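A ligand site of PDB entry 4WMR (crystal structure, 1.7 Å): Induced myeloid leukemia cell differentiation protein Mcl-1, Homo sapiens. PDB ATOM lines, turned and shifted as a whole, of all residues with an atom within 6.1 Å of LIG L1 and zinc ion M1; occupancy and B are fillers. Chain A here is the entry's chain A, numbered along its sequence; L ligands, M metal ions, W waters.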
ATOM      1  N   VAL A  49      18.127  26.245  -5.040  1.00  0.00           N
ATOM      2  CA  VAL A  49      16.912  25.484  -4.739  1.00  0.00           C
ATOM      3  C   VAL A  49      16.155  25.139  -6.028  1.00  0.00           C
ATOM      4  O   VAL A  49      15.754  23.999  -6.226  1.00  0.00           O
ATOM      5  CB  VAL A  49      16.017  26.217  -3.705  1.00  0.00           C
ATOM      6  CG1 VAL A  49      14.653  25.545  -3.580  1.00  0.00           C
ATOM      7  CG2 VAL A  49      16.690  26.242  -2.360  1.00  0.00           C
ATOM      8  N   ASN A  52      18.323  22.478  -7.908  1.00  0.00           N
ATOM      9  CA  ASN A  52      18.468  21.188  -7.230  1.00  0.00           C
ATOM     10  C   ASN A  52      17.158  20.482  -6.957  1.00  0.00           C
ATOM     11  O   ASN A  52      17.136  19.284  -6.699  1.00  0.00           O
ATOM     12  CB  ASN A  52      19.248  21.356  -5.926  1.00  0.00           C
ATOM     13  CG  ASN A  52      20.691  21.755  -6.176  1.00  0.00           C
ATOM     14  OD1 ASN A  52      21.323  21.292  -7.134  1.00  0.00           O
ATOM     15  ND2 ASN A  52      21.220  22.608  -5.309  1.00  0.00           N
ATOM     16  N   HIS A  53      16.066  21.239  -6.989  1.00  0.00           N
ATOM     17  CA  HIS A  53      14.735  20.682  -6.798  1.00  0.00           C
ATOM     18  C   HIS A  53      13.874  20.934  -8.032  1.00  0.00           C
ATOM     19  O   HIS A  53      12.644  21.017  -7.932  1.00  0.00           O
ATOM     20  CB  HIS A  53      14.101  21.308  -5.556  1.00  0.00           C
ATOM     21  CG  HIS A  53      14.933  21.138  -4.328  1.00  0.00           C
ATOM     22  ND1 HIS A  53      14.693  20.152  -3.397  1.00  0.00           N
ATOM     23  CD2 HIS A  53      16.012  21.819  -3.879  1.00  0.00           C
ATOM     24  CE1 HIS A  53      15.588  20.234  -2.422  1.00  0.00           C
ATOM     25  NE2 HIS A  53      16.402  21.240  -2.690  1.00  0.00           N
ATOM     26  N   ALA A  56      10.831  18.441  -8.746  1.00  0.00           N
ATOM     27  CA  ALA A  56       9.650  18.730  -7.920  1.00  0.00           C
ATOM     28  C   ALA A  56       8.982  20.041  -8.322  1.00  0.00           C
ATOM     29  O   ALA A  56       7.751  20.118  -8.374  1.00  0.00           O
ATOM     30  CB  ALA A  56      10.030  18.775  -6.459  1.00  0.00           C
ATOM     31  N   PHE A  57       9.779  21.070  -8.598  1.00  0.00           N
ATOM     32  CA  PHE A  57       9.221  22.363  -8.991  1.00  0.00           C
ATOM     33  C   PHE A  57       8.436  22.272 -10.302  1.00  0.00           C
ATOM     34  O   PHE A  57       7.322  22.795 -10.398  1.00  0.00           O
ATOM     35  CB  PHE A  57      10.323  23.439  -9.078  1.00  0.00           C
ATOM     36  CG  PHE A  57      10.661  24.102  -7.760  1.00  0.00           C
ATOM     37  CD1 PHE A  57      10.361  23.494  -6.529  1.00  0.00           C
ATOM     38  CD2 PHE A  57      11.313  25.325  -7.740  1.00  0.00           C
ATOM     39  CE1 PHE A  57      10.690  24.122  -5.344  1.00  0.00           C
ATOM     40  CE2 PHE A  57      11.653  25.944  -6.552  1.00  0.00           C
ATOM     41  CZ  PHE A  57      11.340  25.344  -5.347  1.00  0.00           C
ATOM     42  N   MET A  60       5.210  20.343  -9.610  1.00  0.00           N
ATOM     43  CA  MET A  60       4.246  21.140  -8.835  1.00  0.00           C
ATOM     44  C   MET A  60       3.583  22.166  -9.748  1.00  0.00           C
ATOM     45  O   MET A  60       2.381  22.402  -9.647  1.00  0.00           O
ATOM     46  CB  MET A  60       4.932  21.841  -7.676  1.00  0.00           C
ATOM     47  CG  MET A  60       3.972  22.483  -6.696  1.00  0.00           C
ATOM     48  SD  MET A  60       2.935  21.269  -5.862  1.00  0.00           S
ATOM     49  CE  MET A  60       1.965  22.365  -4.850  1.00  0.00           C
ATOM     50  N   LEU A  64      -0.486  22.646 -10.496  1.00  0.00           N
ATOM     51  CA  LEU A  64      -1.240  23.885 -10.287  1.00  0.00           C
ATOM     52  C   LEU A  64      -1.958  24.329 -11.566  1.00  0.00           C
ATOM     53  O   LEU A  64      -2.959  25.048 -11.493  1.00  0.00           O
ATOM     54  CB  LEU A  64      -0.318  24.981  -9.769  1.00  0.00           C
ATOM     55  CG  LEU A  64       0.311  24.692  -8.397  1.00  0.00           C
ATOM     56  CD1 LEU A  64       1.462  25.649  -8.117  1.00  0.00           C
ATOM     57  CD2 LEU A  64      -0.713  24.731  -7.276  1.00  0.00           C
ATOM     58  N   LEU A  75      -4.220  28.686  -6.040  1.00  0.00           N
ATOM     59  CA  LEU A  75      -2.930  28.177  -5.540  1.00  0.00           C
ATOM     60  C   LEU A  75      -2.594  28.722  -4.142  1.00  0.00           C
ATOM     61  O   LEU A  75      -1.767  28.150  -3.433  1.00  0.00           O
ATOM     62  CB  LEU A  75      -1.810  28.395  -6.558  1.00  0.00           C
ATOM     63  CG  LEU A  75      -1.348  29.815  -6.881  1.00  0.00           C
ATOM     64  CD1 LEU A  75      -0.470  30.374  -5.769  1.00  0.00           C
ATOM     65  CD2 LEU A  75      -0.604  29.872  -8.204  1.00  0.00           C
ATOM     66  N   SER A  76      -3.237  29.826  -3.741  1.00  0.00           N
ATOM     67  CA  SER A  76      -3.067  30.378  -2.398  1.00  0.00           C
ATOM     68  C   SER A  76      -3.513  29.388  -1.309  1.00  0.00           C
ATOM     69  O   SER A  76      -2.931  29.319  -0.227  1.00  0.00           O
ATOM     70  CB  SER A  76      -3.856  31.689  -2.253  1.00  0.00           C
ATOM     71  OG  SER A  76      -3.611  32.294  -1.000  1.00  0.00           O
ATOM     72  N   VAL A  78      -3.392  26.118  -1.605  1.00  0.00           N
ATOM     73  CA  VAL A  78      -2.370  25.078  -1.594  1.00  0.00           C
ATOM     74  C   VAL A  78      -1.117  25.594  -0.878  1.00  0.00           C
ATOM     75  O   VAL A  78      -0.553  24.897  -0.044  1.00  0.00           O
ATOM     76  CB  VAL A  78      -2.009  24.606  -3.011  1.00  0.00           C
ATOM     77  CG1 VAL A  78      -0.963  23.512  -2.971  1.00  0.00           C
ATOM     78  CG2 VAL A  78      -3.272  24.097  -3.709  1.00  0.00           C
ATOM     79  N   MET A  79      -0.719  26.826  -1.194  1.00  0.00           N
ATOM     80  CA  MET A  79       0.452  27.461  -0.573  1.00  0.00           C
ATOM     81  C   MET A  79       0.320  27.497   0.953  1.00  0.00           C
ATOM     82  O   MET A  79       1.211  27.064   1.662  1.00  0.00           O
ATOM     83  CB  MET A  79       0.635  28.875  -1.132  1.00  0.00           C
ATOM     84  CG  MET A  79       1.825  29.666  -0.587  1.00  0.00           C
ATOM     85  SD  MET A  79       1.589  31.453  -0.716  1.00  0.00           S
ATOM     86  CE  MET A  79       1.238  31.610  -2.464  1.00  0.00           C
ATOM     87  N   ILE A  80      -0.813  27.972   1.454  1.00  0.00           N
ATOM     88  CA  ILE A  80      -0.948  28.133   2.905  1.00  0.00           C
ATOM     89  C   ILE A  80      -0.973  26.756   3.582  1.00  0.00           C
ATOM     90  O   ILE A  80      -0.424  26.588   4.661  1.00  0.00           O
ATOM     91  CB  ILE A  80      -2.154  29.028   3.309  1.00  0.00           C
ATOM     92  CG1 ILE A  80      -2.028  29.421   4.798  1.00  0.00           C
ATOM     93  CG2 ILE A  80      -3.488  28.353   3.024  1.00  0.00           C
ATOM     94  CD1 ILE A  80      -3.073  30.424   5.249  1.00  0.00           C
ATOM     95  N   VAL A  82       0.523  23.724   2.416  1.00  0.00           N
ATOM     96  CA  VAL A  82       1.815  23.053   2.353  1.00  0.00           C
ATOM     97  C   VAL A  82       2.823  23.744   3.269  1.00  0.00           C
ATOM     98  O   VAL A  82       3.608  23.078   3.957  1.00  0.00           O
ATOM     99  CB  VAL A  82       2.337  22.995   0.906  1.00  0.00           C
ATOM    100  CG1 VAL A  82       3.761  22.488   0.853  1.00  0.00           C
ATOM    101  CG2 VAL A  82       1.437  22.092   0.079  1.00  0.00           C
ATOM    102  N   PHE A  83       2.811  25.077   3.280  1.00  0.00           N
ATOM    103  CA  PHE A  83       3.772  25.823   4.074  1.00  0.00           C
ATOM    104  C   PHE A  83       3.501  25.687   5.568  1.00  0.00           C
ATOM    105  O   PHE A  83       4.445  25.591   6.358  1.00  0.00           O
ATOM    106  CB  PHE A  83       3.809  27.301   3.666  1.00  0.00           C
ATOM    107  CG  PHE A  83       4.877  28.088   4.385  1.00  0.00           C
ATOM    108  CD1 PHE A  83       6.229  27.837   4.148  1.00  0.00           C
ATOM    109  CD2 PHE A  83       4.543  29.076   5.305  1.00  0.00           C
ATOM    110  CE1 PHE A  83       7.209  28.549   4.806  1.00  0.00           C
ATOM    111  CE2 PHE A  83       5.528  29.786   5.971  1.00  0.00           C
ATOM    112  CZ  PHE A  83       6.859  29.524   5.717  1.00  0.00           C
ATOM    113  N   ASP A  85       2.043  23.214   7.150  1.00  0.00           N
ATOM    114  CA  ASP A  85       2.301  21.872   7.641  1.00  0.00           C
ATOM    115  C   ASP A  85       3.748  21.768   8.134  1.00  0.00           C
ATOM    116  O   ASP A  85       4.676  22.265   7.497  1.00  0.00           O
ATOM    117  CB  ASP A  85       2.052  20.819   6.549  1.00  0.00           C
ATOM    118  CG  ASP A  85       0.595  20.378   6.467  1.00  0.00           C
ATOM    119  OD1 ASP A  85      -0.281  20.982   7.126  1.00  0.00           O
ATOM    120  OD2 ASP A  85       0.334  19.411   5.745  1.00  0.00           O
ATOM    121  N   ARG A  92      12.834  26.084   4.435  1.00  0.00           N
ATOM    122  CA  ARG A  92      11.468  26.005   3.925  1.00  0.00           C
ATOM    123  C   ARG A  92      10.940  27.347   3.463  1.00  0.00           C
ATOM    124  O   ARG A  92      10.155  27.421   2.517  1.00  0.00           O
ATOM    125  CB  ARG A  92      10.551  25.393   4.972  1.00  0.00           C
ATOM    126  CG  ARG A  92      10.843  23.913   5.158  1.00  0.00           C
ATOM    127  CD  ARG A  92       9.760  23.251   5.971  1.00  0.00           C
ATOM    128  NE  ARG A  92       8.477  23.290   5.295  1.00  0.00           N
ATOM    129  CZ  ARG A  92       7.310  23.063   5.881  1.00  0.00           C
ATOM    130  NH1 ARG A  92       7.245  22.783   7.192  1.00  0.00           N
ATOM    131  NH2 ARG A  92       6.201  23.109   5.156  1.00  0.00           N
ATOM    132  N   THR A  95      12.321  27.759   0.105  1.00  0.00           N
ATOM    133  CA  THR A  95      11.535  26.942  -0.832  1.00  0.00           C
ATOM    134  C   THR A  95      10.241  27.669  -1.226  1.00  0.00           C
ATOM    135  O   THR A  95       9.888  27.728  -2.402  1.00  0.00           O
ATOM    136  CB  THR A  95      11.241  25.545  -0.284  1.00  0.00           C
ATOM    137  OG1 THR A  95      12.471  24.901   0.076  1.00  0.00           O
ATOM    138  CG2 THR A  95      10.538  24.677  -1.313  1.00  0.00           C
ATOM    139  N   LEU A  96       9.553  28.225  -0.223  1.00  0.00           N
ATOM    140  CA  LEU A  96       8.367  29.043  -0.445  1.00  0.00           C
ATOM    141  C   LEU A  96       8.631  30.169  -1.447  1.00  0.00           C
ATOM    142  O   LEU A  96       7.915  30.326  -2.447  1.00  0.00           O
ATOM    143  CB  LEU A  96       7.888  29.621   0.880  1.00  0.00           C
ATOM    144  CG  LEU A  96       6.740  30.629   0.850  1.00  0.00           C
ATOM    145  CD1 LEU A  96       5.430  29.925   0.567  1.00  0.00           C
ATOM    146  CD2 LEU A  96       6.649  31.419   2.166  1.00  0.00           C
ATOM    147  N   ILE A  97       9.662  30.964  -1.183  1.00  0.00           N
ATOM    148  CA  ILE A  97       9.906  32.139  -1.986  1.00  0.00           C
ATOM    149  C   ILE A  97      10.467  31.770  -3.377  1.00  0.00           C
ATOM    150  O   ILE A  97      10.028  32.345  -4.369  1.00  0.00           O
ATOM    151  CB  ILE A  97      10.830  33.120  -1.227  1.00  0.00           C
ATOM    152  CG1 ILE A  97      10.120  33.592   0.051  1.00  0.00           C
ATOM    153  CG2 ILE A  97      11.199  34.286  -2.129  1.00  0.00           C
ATOM    154  CD1 ILE A  97      11.028  34.200   1.094  1.00  0.00           C
ATOM    155  N   PHE A  99      10.020  28.944  -5.003  1.00  0.00           N
ATOM    156  CA  PHE A  99       8.925  28.433  -5.807  1.00  0.00           C
ATOM    157  C   PHE A  99       8.037  29.553  -6.312  1.00  0.00           C
ATOM    158  O   PHE A  99       7.591  29.519  -7.459  1.00  0.00           O
ATOM    159  CB  PHE A  99       8.106  27.363  -5.104  1.00  0.00           C
ATOM    160  CG  PHE A  99       7.133  26.683  -6.022  1.00  0.00           C
ATOM    161  CD1 PHE A  99       7.587  25.912  -7.082  1.00  0.00           C
ATOM    162  CD2 PHE A  99       5.770  26.853  -5.874  1.00  0.00           C
ATOM    163  CE1 PHE A  99       6.698  25.310  -7.947  1.00  0.00           C
ATOM    164  CE2 PHE A  99       4.875  26.243  -6.739  1.00  0.00           C
ATOM    165  CZ  PHE A  99       5.349  25.482  -7.783  1.00  0.00           C
ATOM    166  N   GLY A 100       7.795  30.556  -5.480  1.00  0.00           N
ATOM    167  CA  GLY A 100       7.116  31.787  -5.914  1.00  0.00           C
ATOM    168  C   GLY A 100       7.753  32.372  -7.156  1.00  0.00           C
ATOM    169  O   GLY A 100       7.062  32.748  -8.110  1.00  0.00           O
ATOM    170  N   ALA A 101       9.088  32.452  -7.164  1.00  0.00           N
ATOM    171  CA  ALA A 101       9.821  32.983  -8.320  1.00  0.00           C
ATOM    172  C   ALA A 101       9.626  32.095  -9.549  1.00  0.00           C
ATOM    173  O   ALA A 101       9.465  32.585 -10.671  1.00  0.00           O
ATOM    174  CB  ALA A 101      11.298  33.122  -7.997  1.00  0.00           C
ATOM    175  N   VAL A 103       7.032  30.158 -10.146  1.00  0.00           N
ATOM    176  CA  VAL A 103       5.679  30.455 -10.612  1.00  0.00           C
ATOM    177  C   VAL A 103       5.649  31.795 -11.344  1.00  0.00           C
ATOM    178  O   VAL A 103       5.013  31.916 -12.395  1.00  0.00           O
ATOM    179  CB  VAL A 103       4.659  30.456  -9.447  1.00  0.00           C
ATOM    180  CG1 VAL A 103       3.290  30.887  -9.934  1.00  0.00           C
ATOM    181  CG2 VAL A 103       4.572  29.047  -8.842  1.00  0.00           C
ATOM    182  N   LEU A 119       0.677  37.661  -6.274  1.00  0.00           N
ATOM    183  CA  LEU A 119       1.318  36.448  -5.793  1.00  0.00           C
ATOM    184  C   LEU A 119       2.329  36.773  -4.693  1.00  0.00           C
ATOM    185  O   LEU A 119       2.381  36.085  -3.673  1.00  0.00           O
ATOM    186  CB  LEU A 119       1.988  35.701  -6.940  1.00  0.00           C
ATOM    187  CG  LEU A 119       2.730  34.394  -6.619  1.00  0.00           C
ATOM    188  CD1 LEU A 119       1.766  33.336  -6.085  1.00  0.00           C
ATOM    189  CD2 LEU A 119       3.457  33.911  -7.863  1.00  0.00           C
ATOM    190  N   ILE A 123       2.288  35.385  -0.800  1.00  0.00           N
ATOM    191  CA  ILE A 123       3.446  34.741  -0.161  1.00  0.00           C
ATOM    192  C   ILE A 123       3.845  35.484   1.118  1.00  0.00           C
ATOM    193  O   ILE A 123       4.043  34.877   2.173  1.00  0.00           O
ATOM    194  CB  ILE A 123       4.639  34.660  -1.147  1.00  0.00           C
ATOM    195  CG1 ILE A 123       4.290  33.714  -2.307  1.00  0.00           C
ATOM    196  CG2 ILE A 123       5.914  34.207  -0.448  1.00  0.00           C
ATOM    197  CD1 ILE A 123       5.242  33.788  -3.484  1.00  0.00           C
HETATM  198  C1  LIG L   1       4.263  19.970  -2.593  1.00  0.00           C
HETATM  199  C2  LIG L   1       5.564  19.272  -2.854  1.00  0.00           C
HETATM  200  C3  LIG L   1       5.532  17.902  -3.006  1.00  0.00           C
HETATM  201  C4  LIG L   1       6.701  17.214  -3.257  1.00  0.00           C
HETATM  202  N1  LIG L   1       7.847  17.886  -3.343  1.00  0.00           N
HETATM  203  C5  LIG L   1       7.952  19.251  -3.206  1.00  0.00           C
HETATM  204  C6  LIG L   1       6.783  19.953  -2.928  1.00  0.00           C
HETATM  205  C7  LIG L   1       6.790  21.451  -2.804  1.00  0.00           C
HETATM  206  C8  LIG L   1       6.602  22.118  -4.007  1.00  0.00           C
HETATM  207  C9  LIG L   1       6.571  23.512  -4.083  1.00  0.00           C
HETATM  208  C10 LIG L   1       6.755  24.280  -2.944  1.00  0.00           C
HETATM  209  C11 LIG L   1       6.949  23.608  -1.746  1.00  0.00           C
HETATM  210  C12 LIG L   1       7.147  24.152  -0.396  1.00  0.00           C
HETATM  211  C13 LIG L   1       7.185  25.591   0.030  1.00  0.00           C
HETATM  212  C14 LIG L   1       5.812  25.985   0.624  1.00  0.00           C
HETATM  213  C15 LIG L   1       4.641  25.819  -0.323  1.00  0.00           C
HETATM  214  O1  LIG L   1       4.740  26.729  -1.405  1.00  0.00           O
HETATM  215  C16 LIG L   1       3.804  26.811  -2.389  1.00  0.00           C
HETATM  216  C17 LIG L   1       2.840  25.810  -2.566  1.00  0.00           C
HETATM  217  C18 LIG L   1       1.890  25.952  -3.571  1.00  0.00           C
HETATM  218  C19 LIG L   1       1.898  27.074  -4.402  1.00  0.00           C
HETATM  219  C20 LIG L   1       2.871  28.056  -4.212  1.00  0.00           C
HETATM  220  C21 LIG L   1       2.894  29.181  -5.026  1.00  0.00           C
HETATM  221  C22 LIG L   1       3.859  30.169  -4.853  1.00  0.00           C
HETATM  222  C23 LIG L   1       4.810  30.027  -3.849  1.00  0.00           C
HETATM  223  C24 LIG L   1       4.783  28.918  -3.016  1.00  0.00           C
HETATM  224  C25 LIG L   1       3.828  27.923  -3.208  1.00  0.00           C
HETATM  225  C26 LIG L   1       7.274  22.944   0.411  1.00  0.00           C
HETATM  226  C27 LIG L   1       7.544  23.044   1.863  1.00  0.00           C
HETATM  227  O2  LIG L   1       8.356  22.212   2.323  1.00  0.00           O
HETATM  228  O3  LIG L   1       7.062  23.945   2.572  1.00  0.00           O
HETATM  229  N2  LIG L   1       7.176  21.843  -0.366  1.00  0.00           N
HETATM  230  C28 LIG L   1       7.212  20.490   0.150  1.00  0.00           C
HETATM  231  C29 LIG L   1       8.546  19.824   0.080  1.00  0.00           C
HETATM  232  O4  LIG L   1       9.518  20.450  -0.294  1.00  0.00           O
HETATM  233  N3  LIG L   1       8.564  18.540   0.441  1.00  0.00           N
HETATM  234  C30 LIG L   1       7.556  17.950   1.343  1.00  0.00           C
HETATM  235  C31 LIG L   1       7.194  16.593   0.767  1.00  0.00           C
HETATM  236  N4  LIG L   1       8.366  15.754   0.815  1.00  0.00           N
HETATM  237  C32 LIG L   1       9.677  16.340   0.666  1.00  0.00           C
HETATM  238  C33 LIG L   1       9.627  17.669  -0.082  1.00  0.00           C
HETATM  239  C34 LIG L   1       6.971  22.222  -1.651  1.00  0.00           C
HETATM  240  N5  LIG L   1       9.231  19.689  -3.304  1.00  0.00           N
HETATM  241  C35 LIG L   1       9.627  20.967  -3.431  1.00  0.00           C
HETATM  242  C36 LIG L   1      11.012  20.911  -3.449  1.00  0.00           C
HETATM  243  N6  LIG L   1      11.367  19.606  -3.319  1.00  0.00           N
HETATM  244  C37 LIG L   1      10.262  18.843  -3.224  1.00  0.00           C
HETATM  245  P1  LG2 L   2      14.076  15.979  -3.824  1.00  0.00           P
HETATM  246  O1  LG2 L   2      15.274  15.481  -4.609  1.00  0.00           O
HETATM  247  O2  LG2 L   2      13.589  17.327  -4.316  1.00  0.00           O
HETATM  248  O3  LG2 L   2      13.007  14.934  -3.605  1.00  0.00           O
HETATM  249  O4  LG2 L   2      14.707  16.200  -2.362  1.00  0.00           O
HETATM  250  P2  LG2 L   2      13.929  16.760  -1.069  1.00  0.00           P
HETATM  251  O5  LG2 L   2      15.064  16.903  -0.088  1.00  0.00           O
HETATM  252  O6  LG2 L   2      13.329  18.082  -1.490  1.00  0.00           O
HETATM  253  O7  LG2 L   2      12.900  15.732  -0.655  1.00  0.00           O
HETATM  254 ZN    ZN M   1      13.182  18.785  -3.189  1.00  0.00          ZN
HETATM  255 ZN    ZN M   2      12.130  14.501  -2.033  1.00  0.00          ZN
HETATM  256  O   HOH W   1      12.182  20.509  -0.154  1.00  0.00           O
HETATM  257  O   HOH W   2      11.198  22.868   1.811  1.00  0.00           O
HETATM  258  O   HOH W   3       9.250  20.227   3.849  1.00  0.00           O
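Water W3 bridges an oxygen (O2) of LIG L1 (2.7 Å) and the guanidinium group of Arg 92 (3.5 Å). Water W2 lies within hydrogen-bond range of OG1 of Thr 95 (3.0 Å) and O2 of LIG L1 (3.0 Å).
Zinc ion M1 is bound by an oxygen (O6) of LG2 L2 (1.8 Å), an oxygen (O2) of LG2 L2 (1.9 Å), a nitrogen (N6) of LIG L1 (2.0 Å) and a ring nitrogen (ND1) of His 53 (2.0 Å). Zinc ion M1 has four donor atoms within binding distance.
Of the 25 residues printed, 1 comes within 4 Å of zinc ion M1. The nearest printed residue that does not touch zinc ion M1 is Ala 56 (4.5 Å).
The backbone carbonyl oxygen (O) of Val 82 lies within hydrogen-bond range of the guanidinium group (NH2) of Arg 92 (2.9 Å). NH2 of Arg 92 lies within hydrogen-bond range of O of Phe 83. The backbone carbonyl oxygen (O) of Asp 85 sits at hydrogen-bond distance from the guanidinium group (NH1) of Arg 92, at 2.6 Å.
O3 of LIG L1 lies within salt-bridge range of NH2 of Arg 92, 2.8 Å away.
Merely in contact with LIG L1: Ala 56 (3.2 Å), Leu 96 (3.4 Å), Gly 100 (3.4 Å), Phe 99 (3.5 Å), Met 79 (3.5 Å), Thr 95 (3.6 Å), Val 82 (3.6 Å), Leu 75 (3.6 Å), Phe 57 (3.7 Å), Met 60 (3.8 Å), Val 78 (3.8 Å), Ile 123 (3.8 Å), Phe 83 (3.9 Å) and Leu 119 (3.99 Å). Within 4 Å of LIG L1: His 53, Ala 56, Phe 57, Met 60, Leu 75, Val 78, Met 79, Val 82, Phe 83, Arg 92, Thr 95, Leu 96, Phe 99, Gly 100, Leu 119 and Ile 123. The nearest printed residue that does not touch LIG L1 is Leu 64 (4.003 Å).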
